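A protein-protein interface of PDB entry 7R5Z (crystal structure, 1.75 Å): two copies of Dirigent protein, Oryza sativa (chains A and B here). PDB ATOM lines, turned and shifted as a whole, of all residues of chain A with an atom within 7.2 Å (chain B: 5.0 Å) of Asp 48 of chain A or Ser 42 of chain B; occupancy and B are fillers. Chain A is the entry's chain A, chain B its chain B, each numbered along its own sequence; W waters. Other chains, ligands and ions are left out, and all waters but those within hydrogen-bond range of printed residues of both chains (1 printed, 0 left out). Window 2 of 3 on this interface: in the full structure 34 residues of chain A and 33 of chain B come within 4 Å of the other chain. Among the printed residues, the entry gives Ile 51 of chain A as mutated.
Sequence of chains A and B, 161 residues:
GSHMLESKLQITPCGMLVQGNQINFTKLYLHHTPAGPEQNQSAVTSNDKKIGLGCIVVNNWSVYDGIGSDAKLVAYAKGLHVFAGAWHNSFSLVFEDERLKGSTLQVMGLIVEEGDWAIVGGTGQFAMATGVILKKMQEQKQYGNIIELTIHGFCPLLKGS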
ATOM      1  N   THR A  45     -22.309  13.792 -22.309  1.00  0.00           N
ATOM      2  CA  THR A  45     -22.830  15.132 -22.513  1.00  0.00           C
ATOM      3  C   THR A  45     -24.339  15.075 -22.349  1.00  0.00           C
ATOM      4  O   THR A  45     -24.945  14.000 -22.302  1.00  0.00           O
ATOM      5  CB  THR A  45     -22.478  15.705 -23.902  1.00  0.00           C
ATOM      6  OG1 THR A  45     -23.118  14.930 -24.927  1.00  0.00           O
ATOM      7  CG2 THR A  45     -20.969  15.720 -24.141  1.00  0.00           C
ATOM      8  N   SER A  46     -24.944  16.250 -22.267  1.00  0.00           N
ATOM      9  CA  SER A  46     -26.372  16.402 -22.053  1.00  0.00           C
ATOM     10  C   SER A  46     -26.991  17.071 -23.269  1.00  0.00           C
ATOM     11  O   SER A  46     -26.306  17.744 -24.043  1.00  0.00           O
ATOM     12  CB  SER A  46     -26.662  17.240 -20.794  1.00  0.00           C
ATOM     13  OG  SER A  46     -26.210  16.585 -19.623  1.00  0.00           O
ATOM     14  N   ASN A  47     -28.293  16.869 -23.449  1.00  0.00           N
ATOM     15  CA  ASN A  47     -29.004  17.658 -24.440  1.00  0.00           C
ATOM     16  C   ASN A  47     -28.897  19.133 -24.086  1.00  0.00           C
ATOM     17  O   ASN A  47     -29.028  19.519 -22.921  1.00  0.00           O
ATOM     18  CB  ASN A  47     -30.477  17.266 -24.502  1.00  0.00           C
ATOM     19  CG  ASN A  47     -30.712  16.014 -25.292  1.00  0.00           C
ATOM     20  OD1 ASN A  47     -29.900  15.636 -26.128  1.00  0.00           O
ATOM     21  ND2 ASN A  47     -31.842  15.359 -25.039  1.00  0.00           N
ATOM     22  N   ASP A  48     -28.653  19.959 -25.098  1.00  0.00           N
ATOM     23  CA  ASP A  48     -28.745  21.400 -24.914  1.00  0.00           C
ATOM     24  C   ASP A  48     -30.187  21.776 -24.604  1.00  0.00           C
ATOM     25  O   ASP A  48     -31.118  21.288 -25.251  1.00  0.00           O
ATOM     26  CB  ASP A  48     -28.245  22.120 -26.165  1.00  0.00           C
ATOM     27  CG  ASP A  48     -28.175  23.619 -25.989  1.00  0.00           C
ATOM     28  OD1 ASP A  48     -29.242  24.264 -26.015  1.00  0.00           O
ATOM     29  OD2 ASP A  48     -27.055  24.152 -25.818  1.00  0.00           O
ATOM     30  N   LYS A  49     -30.372  22.637 -23.602  1.00  0.00           N
ATOM     31  CA  LYS A  49     -31.725  22.957 -23.161  1.00  0.00           C
ATOM     32  C   LYS A  49     -32.536  23.600 -24.279  1.00  0.00           C
ATOM     33  O   LYS A  49     -33.708  23.261 -24.481  1.00  0.00           O
ATOM     34  CB  LYS A  49     -31.679  23.868 -21.934  1.00  0.00           C
ATOM     35  N   LYS A  50     -31.924  24.509 -25.037  1.00  0.00           N
ATOM     36  CA  LYS A  50     -32.707  25.331 -25.951  1.00  0.00           C
ATOM     37  C   LYS A  50     -32.931  24.662 -27.300  1.00  0.00           C
ATOM     38  O   LYS A  50     -33.971  24.893 -27.929  1.00  0.00           O
ATOM     39  CB  LYS A  50     -32.029  26.687 -26.142  1.00  0.00           C
ATOM     40  N   ILE A  51     -31.994  23.829 -27.756  1.00  0.00           N
ATOM     41  CA  ILE A  51     -32.080  23.242 -29.089  1.00  0.00           C
ATOM     42  C   ILE A  51     -32.699  21.849 -29.019  1.00  0.00           C
ATOM     43  O   ILE A  51     -33.335  21.398 -29.979  1.00  0.00           O
ATOM     44  CB  ILE A  51     -30.693  23.228 -29.761  1.00  0.00           C
ATOM     45  CG1 ILE A  51     -30.091  24.633 -29.700  1.00  0.00           C
ATOM     46  CG2 ILE A  51     -30.805  22.814 -31.213  1.00  0.00           C
ATOM     47  CD1 ILE A  51     -28.604  24.655 -29.527  1.00  0.00           C
ATOM     48  N   GLY A  52     -32.550  21.167 -27.886  1.00  0.00           N
ATOM     49  CA  GLY A  52     -33.144  19.850 -27.742  1.00  0.00           C
ATOM     50  C   GLY A  52     -32.400  18.754 -28.482  1.00  0.00           C
ATOM     51  O   GLY A  52     -33.000  17.932 -29.182  1.00  0.00           O
ATOM     52  N   LEU A  53     -31.081  18.750 -28.339  1.00  0.00           N
ATOM     53  CA  LEU A  53     -30.218  17.714 -28.885  1.00  0.00           C
ATOM     54  C   LEU A  53     -28.857  17.894 -28.237  1.00  0.00           C
ATOM     55  O   LEU A  53     -28.577  18.924 -27.614  1.00  0.00           O
ATOM     56  CB  LEU A  53     -30.123  17.779 -30.418  1.00  0.00           C
ATOM     57  CG  LEU A  53     -30.055  19.145 -31.111  1.00  0.00           C
ATOM     58  CD1 LEU A  53     -28.783  19.903 -30.766  1.00  0.00           C
ATOM     59  CD2 LEU A  53     -30.196  18.998 -32.618  1.00  0.00           C
ATOM     60  N   GLY A  54     -28.023  16.877 -28.373  1.00  0.00           N
ATOM     61  CA  GLY A  54     -26.641  17.004 -27.950  1.00  0.00           C
ATOM     62  C   GLY A  54     -26.127  15.937 -27.012  1.00  0.00           C
ATOM     63  O   GLY A  54     -24.924  15.859 -26.769  1.00  0.00           O
ATOM     64  N   CYS A  55     -27.018  15.139 -26.436  1.00  0.00           N
ATOM     65  CA  CYS A  55     -26.562  14.095 -25.538  1.00  0.00           C
ATOM     66  C   CYS A  55     -25.711  13.082 -26.296  1.00  0.00           C
ATOM     67  O   CYS A  55     -26.113  12.581 -27.347  1.00  0.00           O
ATOM     68  CB  CYS A  55     -27.754  13.396 -24.907  1.00  0.00           C
ATOM     69  SG  CYS A  55     -27.269  12.105 -23.779  1.00  0.00           S
ATOM     70  N   GLN B  39     -31.701  27.531 -35.269  1.00  0.00           N
ATOM     71  CA  GLN B  39     -30.514  26.757 -34.941  1.00  0.00           C
ATOM     72  C   GLN B  39     -30.847  25.276 -34.835  1.00  0.00           C
ATOM     73  O   GLN B  39     -31.795  24.894 -34.150  1.00  0.00           O
ATOM     74  CB  GLN B  39     -29.922  27.263 -33.625  1.00  0.00           C
ATOM     75  CG  GLN B  39     -28.777  26.425 -33.101  1.00  0.00           C
ATOM     76  CD  GLN B  39     -27.940  27.164 -32.086  1.00  0.00           C
ATOM     77  OE1 GLN B  39     -28.223  28.313 -31.754  1.00  0.00           O
ATOM     78  NE2 GLN B  39     -26.896  26.513 -31.590  1.00  0.00           N
ATOM     79  N   ASN B  40     -30.080  24.442 -35.541  1.00  0.00           N
ATOM     80  CA  ASN B  40     -30.419  23.029 -35.628  1.00  0.00           C
ATOM     81  C   ASN B  40     -29.225  22.147 -35.284  1.00  0.00           C
ATOM     82  O   ASN B  40     -29.120  21.014 -35.758  1.00  0.00           O
ATOM     83  CB  ASN B  40     -30.984  22.694 -37.009  1.00  0.00           C
ATOM     84  CG  ASN B  40     -30.045  23.074 -38.145  1.00  0.00           C
ATOM     85  OD1 ASN B  40     -28.877  23.374 -37.924  1.00  0.00           O
ATOM     86  ND2 ASN B  40     -30.558  23.049 -39.367  1.00  0.00           N
ATOM     87  N   GLN B  41     -28.333  22.649 -34.435  1.00  0.00           N
ATOM     88  CA  GLN B  41     -27.145  21.926 -34.004  1.00  0.00           C
ATOM     89  C   GLN B  41     -26.651  22.574 -32.719  1.00  0.00           C
ATOM     90  O   GLN B  41     -26.962  23.734 -32.435  1.00  0.00           O
ATOM     91  CB  GLN B  41     -26.040  21.930 -35.077  1.00  0.00           C
ATOM     92  CG  GLN B  41     -25.461  23.332 -35.377  1.00  0.00           C
ATOM     93  CD  GLN B  41     -24.258  23.302 -36.315  1.00  0.00           C
ATOM     94  OE1 GLN B  41     -24.243  22.580 -37.313  1.00  0.00           O
ATOM     95  NE2 GLN B  41     -23.242  24.099 -35.999  1.00  0.00           N
ATOM     96  N   SER B  42     -25.881  21.815 -31.938  1.00  0.00           N
ATOM     97  CA  SER B  42     -25.293  22.357 -30.721  1.00  0.00           C
ATOM     98  C   SER B  42     -23.907  21.787 -30.457  1.00  0.00           C
ATOM     99  O   SER B  42     -23.689  20.578 -30.569  1.00  0.00           O
ATOM    100  CB  SER B  42     -26.186  22.082 -29.502  1.00  0.00           C
ATOM    101  OG  SER B  42     -25.617  22.663 -28.346  1.00  0.00           O
ATOM    102  N   ALA B  43     -22.985  22.663 -30.071  1.00  0.00           N
ATOM    103  CA  ALA B  43     -21.661  22.252 -29.624  1.00  0.00           C
ATOM    104  C   ALA B  43     -21.725  21.769 -28.180  1.00  0.00           C
ATOM    105  O   ALA B  43     -22.279  22.458 -27.317  1.00  0.00           O
ATOM    106  CB  ALA B  43     -20.680  23.418 -29.754  1.00  0.00           C
ATOM    107  N   VAL B  44     -21.172  20.584 -27.914  1.00  0.00           N
ATOM    108  CA  VAL B  44     -21.312  19.945 -26.609  1.00  0.00           C
ATOM    109  C   VAL B  44     -19.982  19.622 -25.936  1.00  0.00           C
ATOM    110  O   VAL B  44     -19.977  19.291 -24.739  1.00  0.00           O
ATOM    111  CB  VAL B  44     -22.190  18.677 -26.700  1.00  0.00           C
ATOM    112  CG1 VAL B  44     -23.559  19.048 -27.256  1.00  0.00           C
ATOM    113  CG2 VAL B  44     -21.531  17.635 -27.561  1.00  0.00           C
ATOM    114  N   ILE B  56     -17.010  19.073 -30.395  1.00  0.00           N
ATOM    115  CA  ILE B  56     -17.971  18.161 -31.014  1.00  0.00           C
ATOM    116  C   ILE B  56     -19.316  18.873 -31.074  1.00  0.00           C
ATOM    117  O   ILE B  56     -19.777  19.417 -30.063  1.00  0.00           O
ATOM    118  CB  ILE B  56     -18.096  16.839 -30.231  1.00  0.00           C
ATOM    119  CG1 ILE B  56     -16.810  16.020 -30.349  1.00  0.00           C
ATOM    120  CG2 ILE B  56     -19.299  16.020 -30.734  1.00  0.00           C
ATOM    121  CD1 ILE B  56     -16.680  14.911 -29.315  1.00  0.00           C
ATOM    122  N   VAL B  57     -19.912  18.913 -32.264  1.00  0.00           N
ATOM    123  CA  VAL B  57     -21.240  19.490 -32.472  1.00  0.00           C
ATOM    124  C   VAL B  57     -22.193  18.374 -32.882  1.00  0.00           C
ATOM    125  O   VAL B  57     -21.850  17.550 -33.736  1.00  0.00           O
ATOM    126  CB  VAL B  57     -21.209  20.578 -33.559  1.00  0.00           C
ATOM    127  CG1 VAL B  57     -22.609  21.083 -33.841  1.00  0.00           C
ATOM    128  CG2 VAL B  57     -20.248  21.701 -33.170  1.00  0.00           C
ATOM    129  N   VAL B  58     -23.401  18.375 -32.311  1.00  0.00           N
ATOM    130  CA  VAL B  58     -24.442  17.412 -32.678  1.00  0.00           C
ATOM    131  C   VAL B  58     -25.467  18.131 -33.546  1.00  0.00           C
ATOM    132  O   VAL B  58     -25.866  19.260 -33.236  1.00  0.00           O
ATOM    133  CB  VAL B  58     -25.090  16.801 -31.427  1.00  0.00           C
ATOM    134  CG1 VAL B  58     -26.262  15.909 -31.816  1.00  0.00           C
ATOM    135  CG2 VAL B  58     -24.043  16.001 -30.663  1.00  0.00           C
HETATM  136  O   HOH W   1     -24.738  22.348 -25.304  1.00  0.00           O
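The side-chain carboxylate (OD2) of Asp 48 of chain A is in hydrogen-bond range of the side-chain hydroxyl (OG) of Ser 42 of chain B (3.3 Å).
SG of Cys 55 of chain A lies within hydrogen-bond range of O of Thr 45 of chain A. The backbone NH (N) of Gly 54 of chain A sits at hydrogen-bond distance from the side-chain amide oxygen (OD1) of Asn 47 of chain A, at 3.2 Å. The side-chain carboxylate of Asp 48 of chain A is in hydrogen-bond range of the backbone NH of Ile 51 of chain A. The backbone NH (N) of Asp 48 of chain A lies within hydrogen-bond range of the backbone carbonyl oxygen (O) of Leu 53 of chain A, at 2.7 Å. NE2 of Gln 39 of chain B is in hydrogen-bond range of O of Gln 41 of chain B (2.9 Å). The backbone carbonyl oxygen (O) of Ile 56 of chain B lies within hydrogen-bond range of the backbone NH (N) of Val 44 of chain B, at 2.8 Å.
Among the printed residues, merely in contact across the chains: Ile 51 of chain A with Gln 39 of chain B, Ile 51 of chain A with Gln 41 of chain B, Gly 54 of chain A with Val 44 of chain B, Ile 51 of chain A with Ser 42 of chain B, Leu 53 of chain A with Ser 42 of chain B, Thr 45 of chain A with Val 44 of chain B, Gly 54 of chain A with Val 58 of chain B, Leu 53 of chain A with Val 58 of chain B, Leu 53 of chain A with Asn 40 of chain B and Leu 53 of chain A with Gln 41 of chain B.
Ser 46 of chain A touches none of the printed residues of chain B. Asn 47 of chain A touches none of the printed residues of chain B. Asp 48 of chain A touches one residue of chain B. Of the printed residues of chain B, Gly 54 of chain A touches Val 44 and Val 58. Printed residues of chain A within 4 Å of Asn 40 of chain B: Leu 53. Of the printed residues of chain A, Gln 41 of chain B touches Ile 51 (3.5 Å) and Leu 53 (3.9 Å). Printed residues of chain A within 4 Å of Ser 42 of chain B: Asp 48 (3.3 Å), Ile 51 (3.5 Å) and Leu 53 (3.6 Å). Of the printed residues of chain A, Val 44 of chain B touches Thr 45 (3.8 Å) and Gly 54 (3.5 Å). Printed residues of chain A within 4 Å of Val 58 of chain B: Leu 53 (3.9 Å) and Gly 54 (3.8 Å). The nearest printed residue of chain B that does not touch Asp 48 of chain A is Ala 43 of chain B (5.3 Å).
Along chain B the printed residues that touch a printed residue of chain A span positions 39 to 58.
No position is printed for both chains.
Water W1 lies within hydrogen-bond range of the side-chain carboxylate of Asp 48 of chain A (3.0 Å), the backbone carbonyl oxygen of Ala 43 of chain B (3.2 Å) and the side-chain hydroxyl of Ser 42 of chain B (3.2 Å).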
